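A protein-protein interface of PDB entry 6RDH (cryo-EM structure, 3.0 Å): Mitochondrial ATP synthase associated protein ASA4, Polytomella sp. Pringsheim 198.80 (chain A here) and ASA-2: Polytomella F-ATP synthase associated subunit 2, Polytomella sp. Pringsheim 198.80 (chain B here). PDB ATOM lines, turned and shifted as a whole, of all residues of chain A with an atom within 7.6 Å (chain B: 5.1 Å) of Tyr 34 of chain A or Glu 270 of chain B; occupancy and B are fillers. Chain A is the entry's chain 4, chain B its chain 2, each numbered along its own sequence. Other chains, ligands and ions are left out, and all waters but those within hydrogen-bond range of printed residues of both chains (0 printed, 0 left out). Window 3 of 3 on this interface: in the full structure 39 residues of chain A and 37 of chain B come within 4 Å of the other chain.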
ATOM      1  N   LYS A  27     -16.626  24.107 -21.254  1.00  0.00           N
ATOM      2  CA  LYS A  27     -17.376  25.095 -20.492  1.00  0.00           C
ATOM      3  C   LYS A  27     -18.871  24.973 -20.744  1.00  0.00           C
ATOM      4  O   LYS A  27     -19.666  25.131 -19.817  1.00  0.00           O
ATOM      5  CB  LYS A  27     -16.876  26.491 -20.838  1.00  0.00           C
ATOM      6  CG  LYS A  27     -15.588  26.850 -20.125  1.00  0.00           C
ATOM      7  CD  LYS A  27     -15.061  28.189 -20.576  1.00  0.00           C
ATOM      8  CE  LYS A  27     -13.982  28.680 -19.637  1.00  0.00           C
ATOM      9  NZ  LYS A  27     -13.648  30.104 -19.896  1.00  0.00           N
ATOM     10  N   SER A  28     -19.269  24.641 -21.973  1.00  0.00           N
ATOM     11  CA  SER A  28     -20.686  24.443 -22.259  1.00  0.00           C
ATOM     12  C   SER A  28     -21.223  23.194 -21.572  1.00  0.00           C
ATOM     13  O   SER A  28     -22.342  23.203 -21.045  1.00  0.00           O
ATOM     14  CB  SER A  28     -20.907  24.362 -23.766  1.00  0.00           C
ATOM     15  OG  SER A  28     -22.276  24.520 -24.084  1.00  0.00           O
ATOM     16  N   TYR A  29     -20.429  22.125 -21.535  1.00  0.00           N
ATOM     17  CA  TYR A  29     -20.851  20.907 -20.852  1.00  0.00           C
ATOM     18  C   TYR A  29     -20.913  21.105 -19.343  1.00  0.00           C
ATOM     19  O   TYR A  29     -21.853  20.641 -18.691  1.00  0.00           O
ATOM     20  CB  TYR A  29     -19.898  19.774 -21.210  1.00  0.00           C
ATOM     21  CG  TYR A  29     -20.076  18.510 -20.413  1.00  0.00           C
ATOM     22  CD1 TYR A  29     -21.160  17.677 -20.637  1.00  0.00           C
ATOM     23  CD2 TYR A  29     -19.141  18.137 -19.459  1.00  0.00           C
ATOM     24  CE1 TYR A  29     -21.315  16.515 -19.922  1.00  0.00           C
ATOM     25  CE2 TYR A  29     -19.286  16.981 -18.744  1.00  0.00           C
ATOM     26  CZ  TYR A  29     -20.373  16.172 -18.976  1.00  0.00           C
ATOM     27  OH  TYR A  29     -20.518  15.014 -18.256  1.00  0.00           O
ATOM     28  N   LEU A  30     -19.931  21.804 -18.773  1.00  0.00           N
ATOM     29  CA  LEU A  30     -19.931  22.085 -17.343  1.00  0.00           C
ATOM     30  C   LEU A  30     -21.064  23.027 -16.963  1.00  0.00           C
ATOM     31  O   LEU A  30     -21.652  22.895 -15.885  1.00  0.00           O
ATOM     32  CB  LEU A  30     -18.586  22.686 -16.941  1.00  0.00           C
ATOM     33  CG  LEU A  30     -17.452  21.823 -16.385  1.00  0.00           C
ATOM     34  CD1 LEU A  30     -17.786  21.343 -15.007  1.00  0.00           C
ATOM     35  CD2 LEU A  30     -17.162  20.639 -17.274  1.00  0.00           C
ATOM     36  N   LYS A  31     -21.406  23.957 -17.851  1.00  0.00           N
ATOM     37  CA  LYS A  31     -22.510  24.867 -17.600  1.00  0.00           C
ATOM     38  C   LYS A  31     -23.848  24.154 -17.714  1.00  0.00           C
ATOM     39  O   LYS A  31     -24.801  24.516 -17.018  1.00  0.00           O
ATOM     40  CB  LYS A  31     -22.426  26.030 -18.583  1.00  0.00           C
ATOM     41  CG  LYS A  31     -22.888  27.364 -18.063  1.00  0.00           C
ATOM     42  CD  LYS A  31     -22.601  28.447 -19.086  1.00  0.00           C
ATOM     43  CE  LYS A  31     -23.293  28.147 -20.411  1.00  0.00           C
ATOM     44  NZ  LYS A  31     -22.986  29.156 -21.456  1.00  0.00           N
ATOM     45  N   SER A  32     -23.943  23.145 -18.581  1.00  0.00           N
ATOM     46  CA  SER A  32     -25.155  22.332 -18.618  1.00  0.00           C
ATOM     47  C   SER A  32     -25.233  21.384 -17.430  1.00  0.00           C
ATOM     48  O   SER A  32     -26.330  20.992 -17.023  1.00  0.00           O
ATOM     49  CB  SER A  32     -25.226  21.544 -19.920  1.00  0.00           C
ATOM     50  OG  SER A  32     -26.380  20.729 -19.936  1.00  0.00           O
ATOM     51  N   LEU A  33     -24.089  20.990 -16.876  1.00  0.00           N
ATOM     52  CA  LEU A  33     -24.109  20.168 -15.674  1.00  0.00           C
ATOM     53  C   LEU A  33     -24.440  20.984 -14.439  1.00  0.00           C
ATOM     54  O   LEU A  33     -24.932  20.430 -13.453  1.00  0.00           O
ATOM     55  CB  LEU A  33     -22.766  19.484 -15.468  1.00  0.00           C
ATOM     56  CG  LEU A  33     -22.400  18.314 -16.364  1.00  0.00           C
ATOM     57  CD1 LEU A  33     -21.239  17.630 -15.719  1.00  0.00           C
ATOM     58  CD2 LEU A  33     -23.555  17.362 -16.558  1.00  0.00           C
ATOM     59  N   TYR A  34     -24.147  22.283 -14.451  1.00  0.00           N
ATOM     60  CA  TYR A  34     -24.506  23.115 -13.307  1.00  0.00           C
ATOM     61  C   TYR A  34     -26.006  23.326 -13.223  1.00  0.00           C
ATOM     62  O   TYR A  34     -26.544  23.515 -12.129  1.00  0.00           O
ATOM     63  CB  TYR A  34     -23.789  24.455 -13.388  1.00  0.00           C
ATOM     64  CG  TYR A  34     -24.047  25.367 -12.219  1.00  0.00           C
ATOM     65  CD1 TYR A  34     -24.795  26.524 -12.373  1.00  0.00           C
ATOM     66  CD2 TYR A  34     -23.541  25.074 -10.963  1.00  0.00           C
ATOM     67  CE1 TYR A  34     -25.025  27.369 -11.312  1.00  0.00           C
ATOM     68  CE2 TYR A  34     -23.766  25.913  -9.893  1.00  0.00           C
ATOM     69  CZ  TYR A  34     -24.512  27.057 -10.074  1.00  0.00           C
ATOM     70  OH  TYR A  34     -24.743  27.895  -9.013  1.00  0.00           O
ATOM     71  N   ALA A  35     -26.699  23.277 -14.354  1.00  0.00           N
ATOM     72  CA  ALA A  35     -28.158  23.296 -14.363  1.00  0.00           C
ATOM     73  C   ALA A  35     -28.730  21.883 -14.278  1.00  0.00           C
ATOM     74  O   ALA A  35     -29.547  21.466 -15.099  1.00  0.00           O
ATOM     75  CB  ALA A  35     -28.662  24.019 -15.604  1.00  0.00           C
ATOM     76  N   GLY A  36     -28.262  21.128 -13.283  1.00  0.00           N
ATOM     77  CA  GLY A  36     -28.928  19.924 -12.827  1.00  0.00           C
ATOM     78  C   GLY A  36     -28.883  18.712 -13.728  1.00  0.00           C
ATOM     79  O   GLY A  36     -29.578  17.736 -13.447  1.00  0.00           O
ATOM     80  N   ALA A  37     -28.094  18.729 -14.796  1.00  0.00           N
ATOM     81  CA  ALA A  37     -28.008  17.540 -15.628  1.00  0.00           C
ATOM     82  C   ALA A  37     -27.104  16.501 -14.975  1.00  0.00           C
ATOM     83  O   ALA A  37     -26.341  16.796 -14.054  1.00  0.00           O
ATOM     84  CB  ALA A  37     -27.494  17.883 -17.021  1.00  0.00           C
ATOM     85  N   ALA B 266     -18.035  29.891  -3.374  1.00  0.00           N
ATOM     86  CA  ALA B 266     -19.352  29.525  -3.891  1.00  0.00           C
ATOM     87  C   ALA B 266     -20.089  30.596  -4.710  1.00  0.00           C
ATOM     88  O   ALA B 266     -20.687  30.227  -5.729  1.00  0.00           O
ATOM     89  CB  ALA B 266     -20.240  29.043  -2.739  1.00  0.00           C
ATOM     90  N   PRO B 267     -20.095  31.899  -4.357  1.00  0.00           N
ATOM     91  CA  PRO B 267     -20.736  32.867  -5.265  1.00  0.00           C
ATOM     92  C   PRO B 267     -19.987  33.084  -6.567  1.00  0.00           C
ATOM     93  O   PRO B 267     -20.581  33.614  -7.514  1.00  0.00           O
ATOM     94  CB  PRO B 267     -20.783  34.155  -4.435  1.00  0.00           C
ATOM     95  CG  PRO B 267     -20.721  33.706  -3.056  1.00  0.00           C
ATOM     96  CD  PRO B 267     -19.758  32.582  -3.091  1.00  0.00           C
ATOM     97  N   ALA B 268     -18.714  32.694  -6.655  1.00  0.00           N
ATOM     98  CA  ALA B 268     -18.024  32.728  -7.938  1.00  0.00           C
ATOM     99  C   ALA B 268     -18.586  31.682  -8.887  1.00  0.00           C
ATOM    100  O   ALA B 268     -18.721  31.932 -10.088  1.00  0.00           O
ATOM    101  CB  ALA B 268     -16.529  32.519  -7.736  1.00  0.00           C
ATOM    102  N   ILE B 269     -18.931  30.509  -8.364  1.00  0.00           N
ATOM    103  CA  ILE B 269     -19.555  29.489  -9.193  1.00  0.00           C
ATOM    104  C   ILE B 269     -21.028  29.796  -9.402  1.00  0.00           C
ATOM    105  O   ILE B 269     -21.618  29.364 -10.398  1.00  0.00           O
ATOM    106  CB  ILE B 269     -19.344  28.106  -8.565  1.00  0.00           C
ATOM    107  CG1 ILE B 269     -17.949  28.034  -7.954  1.00  0.00           C
ATOM    108  CG2 ILE B 269     -19.520  27.012  -9.599  1.00  0.00           C
ATOM    109  CD1 ILE B 269     -17.653  26.740  -7.332  1.00  0.00           C
ATOM    110  N   GLU B 270     -21.647  30.530  -8.476  1.00  0.00           N
ATOM    111  CA  GLU B 270     -23.007  31.001  -8.705  1.00  0.00           C
ATOM    112  C   GLU B 270     -23.051  31.996  -9.857  1.00  0.00           C
ATOM    113  O   GLU B 270     -23.929  31.917 -10.724  1.00  0.00           O
ATOM    114  CB  GLU B 270     -23.563  31.643  -7.433  1.00  0.00           C
ATOM    115  CG  GLU B 270     -23.861  30.677  -6.300  1.00  0.00           C
ATOM    116  CD  GLU B 270     -25.169  29.947  -6.477  1.00  0.00           C
ATOM    117  OE1 GLU B 270     -25.984  30.374  -7.321  1.00  0.00           O
ATOM    118  OE2 GLU B 270     -25.387  28.951  -5.762  1.00  0.00           O
ATOM    119  N   LYS B 271     -22.102  32.931  -9.884  1.00  0.00           N
ATOM    120  CA  LYS B 271     -22.044  33.914 -10.958  1.00  0.00           C
ATOM    121  C   LYS B 271     -21.594  33.273 -12.262  1.00  0.00           C
ATOM    122  O   LYS B 271     -22.240  33.435 -13.301  1.00  0.00           O
ATOM    123  CB  LYS B 271     -21.104  35.054 -10.563  1.00  0.00           C
ATOM    124  CG  LYS B 271     -20.979  36.154 -11.600  1.00  0.00           C
ATOM    125  CD  LYS B 271     -22.288  36.886 -11.787  1.00  0.00           C
ATOM    126  CE  LYS B 271     -22.627  37.718 -10.561  1.00  0.00           C
ATOM    127  NZ  LYS B 271     -23.896  38.478 -10.735  1.00  0.00           N
ATOM    128  N   ALA B 272     -20.494  32.531 -12.223  1.00  0.00           N
ATOM    129  CA  ALA B 272     -19.931  31.894 -13.410  1.00  0.00           C
ATOM    130  C   ALA B 272     -19.660  30.427 -13.112  1.00  0.00           C
ATOM    131  O   ALA B 272     -18.700  30.118 -12.378  1.00  0.00           O
ATOM    132  CB  ALA B 272     -18.655  32.602 -13.846  1.00  0.00           C
ATOM    133  N   PRO B 273     -20.459  29.501 -13.649  1.00  0.00           N
ATOM    134  CA  PRO B 273     -20.241  28.083 -13.324  1.00  0.00           C
ATOM    135  C   PRO B 273     -19.004  27.511 -13.980  1.00  0.00           C
ATOM    136  O   PRO B 273     -18.345  26.639 -13.403  1.00  0.00           O
ATOM    137  CB  PRO B 273     -21.514  27.402 -13.847  1.00  0.00           C
ATOM    138  CG  PRO B 273     -22.442  28.515 -14.254  1.00  0.00           C
ATOM    139  CD  PRO B 273     -21.596  29.691 -14.558  1.00  0.00           C
ATOM    140  N   PRO B 296     -23.618  25.952  -1.054  1.00  0.00           N
ATOM    141  CA  PRO B 296     -24.983  25.917  -1.616  1.00  0.00           C
ATOM    142  C   PRO B 296     -25.338  24.681  -2.433  1.00  0.00           C
ATOM    143  O   PRO B 296     -24.502  23.856  -2.802  1.00  0.00           O
ATOM    144  CB  PRO B 296     -25.013  27.167  -2.497  1.00  0.00           C
ATOM    145  CG  PRO B 296     -24.206  28.125  -1.754  1.00  0.00           C
ATOM    146  CD  PRO B 296     -23.107  27.339  -1.084  1.00  0.00           C
ATOM    147  N   ALA B 298     -26.688  24.023  -5.441  1.00  0.00           N
ATOM    148  CA  ALA B 298     -26.227  23.775  -6.800  1.00  0.00           C
ATOM    149  C   ALA B 298     -24.745  23.446  -6.817  1.00  0.00           C
ATOM    150  O   ALA B 298     -24.311  22.553  -7.554  1.00  0.00           O
ATOM    151  CB  ALA B 298     -26.523  24.979  -7.688  1.00  0.00           C
ATOM    152  N   VAL B 299     -23.963  24.138  -5.983  1.00  0.00           N
ATOM    153  CA  VAL B 299     -22.516  23.955  -5.948  1.00  0.00           C
ATOM    154  C   VAL B 299     -22.149  22.576  -5.415  1.00  0.00           C
ATOM    155  O   VAL B 299     -21.151  21.987  -5.848  1.00  0.00           O
ATOM    156  CB  VAL B 299     -21.873  25.081  -5.118  1.00  0.00           C
ATOM    157  CG1 VAL B 299     -20.373  25.091  -5.280  1.00  0.00           C
ATOM    158  CG2 VAL B 299     -22.450  26.418  -5.523  1.00  0.00           C
ATOM    159  N   PHE B 302     -22.769  20.162  -8.194  1.00  0.00           N
ATOM    160  CA  PHE B 302     -21.824  20.528  -9.241  1.00  0.00           C
ATOM    161  C   PHE B 302     -20.442  19.948  -8.977  1.00  0.00           C
ATOM    162  O   PHE B 302     -19.880  19.258  -9.832  1.00  0.00           O
ATOM    163  CB  PHE B 302     -21.760  22.045  -9.350  1.00  0.00           C
ATOM    164  CG  PHE B 302     -20.975  22.535 -10.517  1.00  0.00           C
ATOM    165  CD1 PHE B 302     -19.896  23.378 -10.330  1.00  0.00           C
ATOM    166  CD2 PHE B 302     -21.321  22.167 -11.800  1.00  0.00           C
ATOM    167  CE1 PHE B 302     -19.174  23.835 -11.399  1.00  0.00           C
ATOM    168  CE2 PHE B 302     -20.599  22.626 -12.873  1.00  0.00           C
ATOM    169  CZ  PHE B 302     -19.527  23.459 -12.671  1.00  0.00           C
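Among the printed residues, merely in contact across the chains: Leu 30 of chain A with Phe 302 of chain B (3.2 Å), Tyr 34 of chain A with Ile 269 of chain B (3.7 Å), Tyr 34 of chain A with Pro 273 of chain B (3.6 Å), Tyr 34 of chain A with Ala 298 of chain B (3.7 Å) and Tyr 34 of chain A with Phe 302 of chain B (3.6 Å).
The side-chain carboxylate (OE1) of Glu 270 of chain B lies within hydrogen-bond range of the side-chain hydroxyl (OH) of Tyr 34 of chain A.
Printed residues of chain A that touch a printed residue of chain B: Leu 30 and Tyr 34.
Hydrophobic or aromatic side chains of chain A that line the printed part of chain B: Leu 30 and Tyr 34.
Among the printed residues, 6 pairs touch across the chains.
Printed residues of chain B within 4 Å of Leu 30 of chain A: Phe 302.
Of the printed residues of chain B, Tyr 34 of chain A touches Ile 269 (3.7 Å), Glu 270 (3.2 Å), Pro 273 (3.6 Å), Ala 298 (3.7 Å) and Phe 302 (3.6 Å).
Glu 270 of chain B touches just one residue of chain A: Tyr 34.
Of the printed residues of chain A, Pro 273 of chain B touches Tyr 34 (3.6 Å).
Printed residues of chain A within 4 Å of Ala 298 of chain B: Tyr 34 (3.7 Å).
Printed residues of chain A within 4 Å of Phe 302 of chain B: Leu 30 and Tyr 34.
The nearest residue of chain B that does not touch Tyr 34 of chain A is Val 299 of chain B (4.3 Å).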
